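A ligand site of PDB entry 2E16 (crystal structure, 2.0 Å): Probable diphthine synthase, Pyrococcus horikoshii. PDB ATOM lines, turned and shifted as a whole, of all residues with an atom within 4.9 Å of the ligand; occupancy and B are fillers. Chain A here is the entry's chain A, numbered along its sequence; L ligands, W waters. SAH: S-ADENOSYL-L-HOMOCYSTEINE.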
ATOM      1  N   LEU A  10      11.447  10.836  12.095  1.00  0.00           N
ATOM      2  CA  LEU A  10      11.639  12.148  12.718  1.00  0.00           C
ATOM      3  C   LEU A  10      11.987  12.353  14.181  1.00  0.00           C
ATOM      4  O   LEU A  10      12.874  13.144  14.505  1.00  0.00           O
ATOM      5  CB  LEU A  10      10.389  12.985  12.450  1.00  0.00           C
ATOM      6  CG  LEU A  10       9.894  13.155  11.006  1.00  0.00           C
ATOM      7  CD1 LEU A  10       8.482  13.698  11.024  1.00  0.00           C
ATOM      8  CD2 LEU A  10      10.835  14.056  10.242  1.00  0.00           C
ATOM      9  N   TYR A  11      11.309  11.642  15.076  1.00  0.00           N
ATOM     10  CA  TYR A  11      11.467  11.890  16.501  1.00  0.00           C
ATOM     11  C   TYR A  11      11.788  10.724  17.443  1.00  0.00           C
ATOM     12  O   TYR A  11      12.707  10.810  18.256  1.00  0.00           O
ATOM     13  CB  TYR A  11      10.203  12.627  16.955  1.00  0.00           C
ATOM     14  CG  TYR A  11      10.175  13.102  18.389  1.00  0.00           C
ATOM     15  CD1 TYR A  11      10.977  14.176  18.806  1.00  0.00           C
ATOM     16  CD2 TYR A  11       9.328  12.516  19.314  1.00  0.00           C
ATOM     17  CE1 TYR A  11      10.904  14.653  20.121  1.00  0.00           C
ATOM     18  CE2 TYR A  11       9.250  12.976  20.625  1.00  0.00           C
ATOM     19  CZ  TYR A  11      10.037  14.036  21.018  1.00  0.00           C
ATOM     20  OH  TYR A  11       9.945  14.491  22.316  1.00  0.00           O
ATOM     21  N   THR A  36      23.720  12.717  11.327  1.00  0.00           N
ATOM     22  CA  THR A  36      23.083  13.520  10.286  1.00  0.00           C
ATOM     23  C   THR A  36      21.869  14.283  10.798  1.00  0.00           C
ATOM     24  O   THR A  36      21.450  15.274  10.211  1.00  0.00           O
ATOM     25  CB  THR A  36      22.637  12.644   9.090  1.00  0.00           C
ATOM     26  OG1 THR A  36      21.791  11.583   9.553  1.00  0.00           O
ATOM     27  CG2 THR A  36      23.847  12.060   8.378  1.00  0.00           C
ATOM     28  N   SER A  37      21.304  13.811  11.907  1.00  0.00           N
ATOM     29  CA  SER A  37      20.152  14.493  12.473  1.00  0.00           C
ATOM     30  C   SER A  37      19.950  14.073  13.915  1.00  0.00           C
ATOM     31  O   SER A  37      20.598  13.148  14.396  1.00  0.00           O
ATOM     32  CB  SER A  37      18.900  14.164  11.655  1.00  0.00           C
ATOM     33  OG  SER A  37      17.812  14.949  12.099  1.00  0.00           O
ATOM     34  N   LEU A  38      19.041  14.757  14.597  1.00  0.00           N
ATOM     35  CA  LEU A  38      18.742  14.456  15.992  1.00  0.00           C
ATOM     36  C   LEU A  38      17.348  13.917  16.199  1.00  0.00           C
ATOM     37  O   LEU A  38      16.360  14.530  15.792  1.00  0.00           O
ATOM     38  CB  LEU A  38      18.923  15.721  16.843  1.00  0.00           C
ATOM     39  CG  LEU A  38      18.595  15.599  18.340  1.00  0.00           C
ATOM     40  CD1 LEU A  38      19.566  14.615  19.011  1.00  0.00           C
ATOM     41  CD2 LEU A  38      18.684  16.960  18.995  1.00  0.00           C
ATOM     42  N   PRO A  85      18.581   8.521  10.984  1.00  0.00           N
ATOM     43  CA  PRO A  85      17.415   9.308  11.405  1.00  0.00           C
ATOM     44  C   PRO A  85      16.693   9.735  10.125  1.00  0.00           C
ATOM     45  O   PRO A  85      17.281   9.705   9.042  1.00  0.00           O
ATOM     46  CB  PRO A  85      18.057  10.498  12.119  1.00  0.00           C
ATOM     47  CG  PRO A  85      19.373   9.963  12.598  1.00  0.00           C
ATOM     48  CD  PRO A  85      19.834   9.156  11.427  1.00  0.00           C
ATOM     49  N   GLY A  86      15.426  10.135  10.252  1.00  0.00           N
ATOM     50  CA  GLY A  86      14.645  10.572   9.109  1.00  0.00           C
ATOM     51  C   GLY A  86      14.687   9.596   7.953  1.00  0.00           C
ATOM     52  O   GLY A  86      14.624   8.391   8.170  1.00  0.00           O
ATOM     53  N   ASP A  87      14.762  10.120   6.732  1.00  0.00           N
ATOM     54  CA  ASP A  87      14.869   9.274   5.534  1.00  0.00           C
ATOM     55  C   ASP A  87      16.365   9.174   5.259  1.00  0.00           C
ATOM     56  O   ASP A  87      17.063  10.186   5.234  1.00  0.00           O
ATOM     57  CB  ASP A  87      14.147   9.921   4.354  1.00  0.00           C
ATOM     58  CG  ASP A  87      14.221   9.073   3.087  1.00  0.00           C
ATOM     59  OD1 ASP A  87      15.332   8.922   2.517  1.00  0.00           O
ATOM     60  OD2 ASP A  87      13.172   8.548   2.670  1.00  0.00           O
ATOM     61  N   VAL A  90      17.905  11.639   2.392  1.00  0.00           N
ATOM     62  CA  VAL A  90      17.498  13.033   2.355  1.00  0.00           C
ATOM     63  C   VAL A  90      18.457  13.933   3.139  1.00  0.00           C
ATOM     64  O   VAL A  90      18.646  13.751   4.342  1.00  0.00           O
ATOM     65  CB  VAL A  90      16.076  13.232   2.939  1.00  0.00           C
ATOM     66  CG1 VAL A  90      15.767  14.713   3.098  1.00  0.00           C
ATOM     67  CG2 VAL A  90      15.043  12.567   2.025  1.00  0.00           C
ATOM     68  N   ALA A  91      19.044  14.907   2.457  1.00  0.00           N
ATOM     69  CA  ALA A  91      19.961  15.847   3.089  1.00  0.00           C
ATOM     70  C   ALA A  91      21.162  15.138   3.727  1.00  0.00           C
ATOM     71  O   ALA A  91      21.701  15.588   4.739  1.00  0.00           O
ATOM     72  CB  ALA A  91      19.235  16.698   4.134  1.00  0.00           C
ATOM     73  N   THR A  92      21.555  14.021   3.127  1.00  0.00           N
ATOM     74  CA  THR A  92      22.736  13.289   3.506  1.00  0.00           C
ATOM     75  C   THR A  92      23.515  12.978   2.246  1.00  0.00           C
ATOM     76  O   THR A  92      23.089  13.272   1.137  1.00  0.00           O
ATOM     77  CB  THR A  92      22.309  11.977   4.202  1.00  0.00           C
ATOM     78  OG1 THR A  92      21.848  11.038   3.229  1.00  0.00           O
ATOM     79  CG2 THR A  92      21.202  12.226   5.248  1.00  0.00           C
ATOM     80  N   PRO A 114       9.559   8.847   7.568  1.00  0.00           N
ATOM     81  CA  PRO A 114       9.169  10.264   7.566  1.00  0.00           C
ATOM     82  C   PRO A 114      10.393  11.178   7.540  1.00  0.00           C
ATOM     83  O   PRO A 114      11.362  10.947   8.265  1.00  0.00           O
ATOM     84  CB  PRO A 114       8.377  10.419   8.868  1.00  0.00           C
ATOM     85  CG  PRO A 114       7.835   9.048   9.102  1.00  0.00           C
ATOM     86  CD  PRO A 114       8.985   8.140   8.730  1.00  0.00           C
ATOM     87  N   SER A 115      10.342  12.211   6.706  1.00  0.00           N
ATOM     88  CA  SER A 115      11.444  13.147   6.560  1.00  0.00           C
ATOM     89  C   SER A 115      10.992  14.571   6.865  1.00  0.00           C
ATOM     90  O   SER A 115       9.861  14.939   6.569  1.00  0.00           O
ATOM     91  CB  SER A 115      11.998  13.092   5.129  1.00  0.00           C
ATOM     92  OG  SER A 115      13.003  14.074   4.933  1.00  0.00           O
ATOM     93  N   ILE A 116      11.888  15.367   7.436  1.00  0.00           N
ATOM     94  CA  ILE A 116      11.549  16.750   7.757  1.00  0.00           C
ATOM     95  C   ILE A 116      11.203  17.490   6.454  1.00  0.00           C
ATOM     96  O   ILE A 116      10.400  18.414   6.445  1.00  0.00           O
ATOM     97  CB  ILE A 116      12.728  17.449   8.469  1.00  0.00           C
ATOM     98  CG1 ILE A 116      12.293  18.816   8.990  1.00  0.00           C
ATOM     99  CG2 ILE A 116      13.919  17.591   7.521  1.00  0.00           C
ATOM    100  CD1 ILE A 116      11.271  18.736  10.113  1.00  0.00           C
ATOM    101  N   TYR A 117      11.803  17.045   5.362  1.00  0.00           N
ATOM    102  CA  TYR A 117      11.568  17.662   4.062  1.00  0.00           C
ATOM    103  C   TYR A 117      10.084  17.683   3.684  1.00  0.00           C
ATOM    104  O   TYR A 117       9.619  18.620   3.045  1.00  0.00           O
ATOM    105  CB  TYR A 117      12.396  16.931   2.998  1.00  0.00           C
ATOM    106  CG  TYR A 117      12.350  17.583   1.632  1.00  0.00           C
ATOM    107  CD1 TYR A 117      12.914  18.844   1.415  1.00  0.00           C
ATOM    108  CD2 TYR A 117      11.757  16.930   0.556  1.00  0.00           C
ATOM    109  CE1 TYR A 117      12.875  19.432   0.140  1.00  0.00           C
ATOM    110  CE2 TYR A 117      11.715  17.489  -0.703  1.00  0.00           C
ATOM    111  CZ  TYR A 117      12.276  18.744  -0.915  1.00  0.00           C
ATOM    112  OH  TYR A 117      12.232  19.274  -2.176  1.00  0.00           O
ATOM    113  N   PHE A 165      17.574  23.927   6.660  1.00  0.00           N
ATOM    114  CA  PHE A 165      18.005  22.913   7.593  1.00  0.00           C
ATOM    115  C   PHE A 165      18.976  23.679   8.490  1.00  0.00           C
ATOM    116  O   PHE A 165      19.654  24.589   8.023  1.00  0.00           O
ATOM    117  CB  PHE A 165      18.752  21.787   6.856  1.00  0.00           C
ATOM    118  CG  PHE A 165      17.859  20.976   5.952  1.00  0.00           C
ATOM    119  CD1 PHE A 165      17.112  19.920   6.458  1.00  0.00           C
ATOM    120  CD2 PHE A 165      17.766  21.277   4.601  1.00  0.00           C
ATOM    121  CE1 PHE A 165      16.270  19.168   5.629  1.00  0.00           C
ATOM    122  CE2 PHE A 165      16.923  20.537   3.753  1.00  0.00           C
ATOM    123  CZ  PHE A 165      16.181  19.485   4.283  1.00  0.00           C
ATOM    124  N   LEU A 166      19.030  23.338   9.776  1.00  0.00           N
ATOM    125  CA  LEU A 166      19.940  24.002  10.702  1.00  0.00           C
ATOM    126  C   LEU A 166      21.119  23.085  11.016  1.00  0.00           C
ATOM    127  O   LEU A 166      20.962  21.862  11.052  1.00  0.00           O
ATOM    128  CB  LEU A 166      19.194  24.425  11.976  1.00  0.00           C
ATOM    129  CG  LEU A 166      17.973  25.313  11.717  1.00  0.00           C
ATOM    130  CD1 LEU A 166      17.428  25.849  13.035  1.00  0.00           C
ATOM    131  CD2 LEU A 166      18.372  26.483  10.801  1.00  0.00           C
ATOM    132  N   ASP A 167      22.289  23.670  11.248  1.00  0.00           N
ATOM    133  CA  ASP A 167      23.485  22.893  11.506  1.00  0.00           C
ATOM    134  C   ASP A 167      23.450  22.008  12.744  1.00  0.00           C
ATOM    135  O   ASP A 167      22.657  22.228  13.673  1.00  0.00           O
ATOM    136  CB  ASP A 167      24.708  23.816  11.585  1.00  0.00           C
ATOM    137  CG  ASP A 167      25.996  23.126  11.163  1.00  0.00           C
ATOM    138  OD1 ASP A 167      25.966  21.898  10.911  1.00  0.00           O
ATOM    139  OD2 ASP A 167      27.036  23.812  11.087  1.00  0.00           O
ATOM    140  N   ILE A 168      24.294  20.995  12.741  1.00  0.00           N
ATOM    141  CA  ILE A 168      24.393  20.050  13.841  1.00  0.00           C
ATOM    142  C   ILE A 168      25.810  19.517  13.982  1.00  0.00           C
ATOM    143  O   ILE A 168      26.476  19.239  12.983  1.00  0.00           O
ATOM    144  CB  ILE A 168      23.425  18.847  13.653  1.00  0.00           C
ATOM    145  CG1 ILE A 168      23.658  17.795  14.738  1.00  0.00           C
ATOM    146  CG2 ILE A 168      23.625  18.232  12.267  1.00  0.00           C
ATOM    147  CD1 ILE A 168      22.775  16.570  14.618  1.00  0.00           C
ATOM    148  N   LEU A 206       9.583  25.293  13.133  1.00  0.00           N
ATOM    149  CA  LEU A 206       9.036  23.979  13.412  1.00  0.00           C
ATOM    150  C   LEU A 206      10.075  23.254  14.247  1.00  0.00           C
ATOM    151  O   LEU A 206      11.204  23.016  13.797  1.00  0.00           O
ATOM    152  CB  LEU A 206       8.784  23.198  12.107  1.00  0.00           C
ATOM    153  CG  LEU A 206       8.279  21.766  12.279  1.00  0.00           C
ATOM    154  CD1 LEU A 206       6.987  21.739  13.110  1.00  0.00           C
ATOM    155  CD2 LEU A 206       8.038  21.143  10.902  1.00  0.00           C
ATOM    156  N   ALA A 207       9.703  22.913  15.478  1.00  0.00           N
ATOM    157  CA  ALA A 207      10.630  22.226  16.375  1.00  0.00           C
ATOM    158  C   ALA A 207      10.098  20.871  16.791  1.00  0.00           C
ATOM    159  O   ALA A 207       8.923  20.738  17.170  1.00  0.00           O
ATOM    160  CB  ALA A 207      10.899  23.086  17.601  1.00  0.00           C
ATOM    161  N   ARG A 208      10.963  19.879  16.712  1.00  0.00           N
ATOM    162  CA  ARG A 208      10.637  18.507  17.078  1.00  0.00           C
ATOM    163  C   ARG A 208       9.464  17.920  16.287  1.00  0.00           C
ATOM    164  O   ARG A 208       8.525  17.361  16.860  1.00  0.00           O
ATOM    165  CB  ARG A 208      10.381  18.409  18.594  1.00  0.00           C
ATOM    166  CG  ARG A 208      11.554  18.919  19.459  1.00  0.00           C
ATOM    167  CD  ARG A 208      11.237  18.880  20.959  1.00  0.00           C
ATOM    168  NE  ARG A 208       9.962  19.527  21.230  1.00  0.00           N
ATOM    169  CZ  ARG A 208       9.748  20.837  21.107  1.00  0.00           C
ATOM    170  NH1 ARG A 208      10.730  21.639  20.732  1.00  0.00           N
ATOM    171  NH2 ARG A 208       8.533  21.325  21.313  1.00  0.00           N
ATOM    172  N   ALA A 209       9.528  18.047  14.969  1.00  0.00           N
ATOM    173  CA  ALA A 209       8.486  17.484  14.117  1.00  0.00           C
ATOM    174  C   ALA A 209       8.551  15.987  14.395  1.00  0.00           C
ATOM    175  O   ALA A 209       9.626  15.450  14.664  1.00  0.00           O
ATOM    176  CB  ALA A 209       8.781  17.771  12.641  1.00  0.00           C
ATOM    177  N   GLY A 210       7.417  15.314  14.309  1.00  0.00           N
ATOM    178  CA  GLY A 210       7.396  13.893  14.577  1.00  0.00           C
ATOM    179  C   GLY A 210       6.819  13.605  15.949  1.00  0.00           C
ATOM    180  O   GLY A 210       6.192  12.572  16.164  1.00  0.00           O
ATOM    181  N   PRO A 233      15.600  19.054  17.641  1.00  0.00           N
ATOM    182  CA  PRO A 233      16.043  19.853  16.496  1.00  0.00           C
ATOM    183  C   PRO A 233      15.026  20.901  16.064  1.00  0.00           C
ATOM    184  O   PRO A 233      13.826  20.779  16.315  1.00  0.00           O
ATOM    185  CB  PRO A 233      16.280  18.797  15.419  1.00  0.00           C
ATOM    186  CG  PRO A 233      15.187  17.804  15.698  1.00  0.00           C
ATOM    187  CD  PRO A 233      15.207  17.695  17.208  1.00  0.00           C
ATOM    188  N   HIS A 234      15.527  21.940  15.390  1.00  0.00           N
ATOM    189  CA  HIS A 234      14.682  23.020  14.896  1.00  0.00           C
ATOM    190  C   HIS A 234      14.905  23.165  13.398  1.00  0.00           C
ATOM    191  O   HIS A 234      15.977  22.846  12.874  1.00  0.00           O
ATOM    192  CB  HIS A 234      15.077  24.360  15.532  1.00  0.00           C
ATOM    193  CG  HIS A 234      14.772  24.477  16.990  1.00  0.00           C
ATOM    194  ND1 HIS A 234      14.992  25.640  17.701  1.00  0.00           N
ATOM    195  CD2 HIS A 234      14.252  23.591  17.871  1.00  0.00           C
ATOM    196  CE1 HIS A 234      14.609  25.468  18.956  1.00  0.00           C
ATOM    197  NE2 HIS A 234      14.159  24.231  19.087  1.00  0.00           N
ATOM    198  N   ILE A 235      13.881  23.668  12.706  1.00  0.00           N
ATOM    199  CA  ILE A 235      14.000  23.927  11.279  1.00  0.00           C
ATOM    200  C   ILE A 235      13.468  25.348  11.109  1.00  0.00           C
ATOM    201  O   ILE A 235      12.561  25.754  11.833  1.00  0.00           O
ATOM    202  CB  ILE A 235      13.141  22.929  10.439  1.00  0.00           C
ATOM    203  CG1 ILE A 235      13.658  22.893   8.994  1.00  0.00           C
ATOM    204  CG2 ILE A 235      11.684  23.343  10.431  1.00  0.00           C
ATOM    205  CD1 ILE A 235      14.900  22.057   8.814  1.00  0.00           C
HETATM  206  N   SAH L   1      17.647  12.714   6.544  1.00  0.00           N
HETATM  207  CA  SAH L   1      17.063  13.703   7.550  1.00  0.00           C
HETATM  208  CB  SAH L   1      17.590  15.106   7.533  1.00  0.00           C
HETATM  209  CG  SAH L   1      19.078  15.340   7.720  1.00  0.00           C
HETATM  210  SD  SAH L   1      19.307  17.151   7.949  1.00  0.00           S
HETATM  211  C   SAH L   1      15.485  13.708   7.326  1.00  0.00           C
HETATM  212  O   SAH L   1      15.003  12.991   6.444  1.00  0.00           O
HETATM  213  OXT SAH L   1      14.803  14.476   8.112  1.00  0.00           O
HETATM  214  C5' SAH L   1      19.092  17.277   9.671  1.00  0.00           C
HETATM  215  C4' SAH L   1      18.492  18.694  10.033  1.00  0.00           C
HETATM  216  O4' SAH L   1      17.118  18.701   9.602  1.00  0.00           O
HETATM  217  C3' SAH L   1      18.501  19.033  11.478  1.00  0.00           C
HETATM  218  O3' SAH L   1      19.718  19.691  11.830  1.00  0.00           O
HETATM  219  C2' SAH L   1      17.219  19.894  11.632  1.00  0.00           C
HETATM  220  O2' SAH L   1      17.449  21.275  11.351  1.00  0.00           O
HETATM  221  C1' SAH L   1      16.211  19.234  10.674  1.00  0.00           C
HETATM  222  N9  SAH L   1      15.476  18.247  11.232  1.00  0.00           N
HETATM  223  C8  SAH L   1      15.512  16.855  11.198  1.00  0.00           C
HETATM  224  N7  SAH L   1      14.586  16.267  11.889  1.00  0.00           N
HETATM  225  C5  SAH L   1      13.832  17.322  12.463  1.00  0.00           C
HETATM  226  C6  SAH L   1      12.673  17.326  13.321  1.00  0.00           C
HETATM  227  N6  SAH L   1      12.069  16.218  13.783  1.00  0.00           N
HETATM  228  N1  SAH L   1      12.212  18.579  13.670  1.00  0.00           N
HETATM  229  C2  SAH L   1      12.788  19.739  13.250  1.00  0.00           C
HETATM  230  N3  SAH L   1      13.886  19.779  12.425  1.00  0.00           N
HETATM  231  C4  SAH L   1      14.351  18.532  12.070  1.00  0.00           C
HETATM  232  O   HOH W   1      20.270  20.871  14.455  1.00  0.00           O
HETATM  233  O   HOH W   2      19.243  11.845   8.487  1.00  0.00           O
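The backbone carbonyl oxygen (O) of Thr 36 sits close to a sulfur (SD) of the ligand (3.6 Å).
O of Pro 85 touches N of the ligand, at 3.9 Å.
Gly 86 touches the ligand.
Ala 91 touches the ligand.
CG2 of Thr 92 touches N of the ligand, at 3.8 Å.
Phe 165 touches the ligand (CD1 to O4', 3.4 Å).
Leu 206 touches the ligand (O to C2, 3.7 Å).
Arg 208 touches the ligand (N to N1, 3.5 Å).
Pro 233 touches the ligand (O to C2, 3.4 Å).
Ile 235 touches the ligand.
Water W2 lies within hydrogen-bond range of N of the ligand (2.7 Å), OG1 of Thr 36 (2.8 Å) and O of Pro 85 (3.0 Å).
Water W1 bridges the backbone carbonyl oxygen (O) of Asp 167 (2.9 Å) and an oxygen (O3') of the ligand (2.9 Å).
The backbone NH (N) of Tyr 117 lies close to the side-chain hydroxyl (OG) of Ser 115 (3.2 Å).
The backbone NH of Arg 208 sits at hydrogen-bond distance from the backbone carbonyl oxygen of Pro 233 (3.0 Å).
O of Leu 206 sits at hydrogen-bond distance from N of Ile 235 (3.0 Å).
N of Leu 166 sits at hydrogen-bond distance from O2' of the ligand.
An oxygen (O3') of the ligand sits at hydrogen-bond distance from the backbone carbonyl oxygen (O) of Leu 166, at 2.6 Å.
The backbone carbonyl oxygen of Val 90 is in hydrogen-bond range of a nitrogen (N) of the ligand (2.6 Å).
O of His 234 sits at hydrogen-bond distance from O2' of the ligand (2.6 Å).
N of Ala 209 sits at hydrogen-bond distance from N1 of the ligand, at 3.0 Å.
A nitrogen (N6) of the ligand lies within hydrogen-bond range of the backbone carbonyl oxygen (O) of Ala 209.
The side-chain hydroxyl (OG) of Ser 115 is in hydrogen-bond range of an oxygen (O) of the ligand, at 2.7 Å.
The backbone NH (N) of Asp 87 is in hydrogen-bond range of an oxygen (O) of the ligand, at 2.9 Å.
O of Asp 87 is in hydrogen-bond range of N of the ligand, at 2.9 Å.
The side-chain hydroxyl (OG) of Ser 37 sits close to a nitrogen (N7) of the ligand (3.5 Å).
OXT of the ligand sits at hydrogen-bond distance from N of Ile 116, 3.1 Å away.
The backbone carbonyl oxygen (O) of Leu 10 is in hydrogen-bond range of a nitrogen (N6) of the ligand (3.3 Å).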
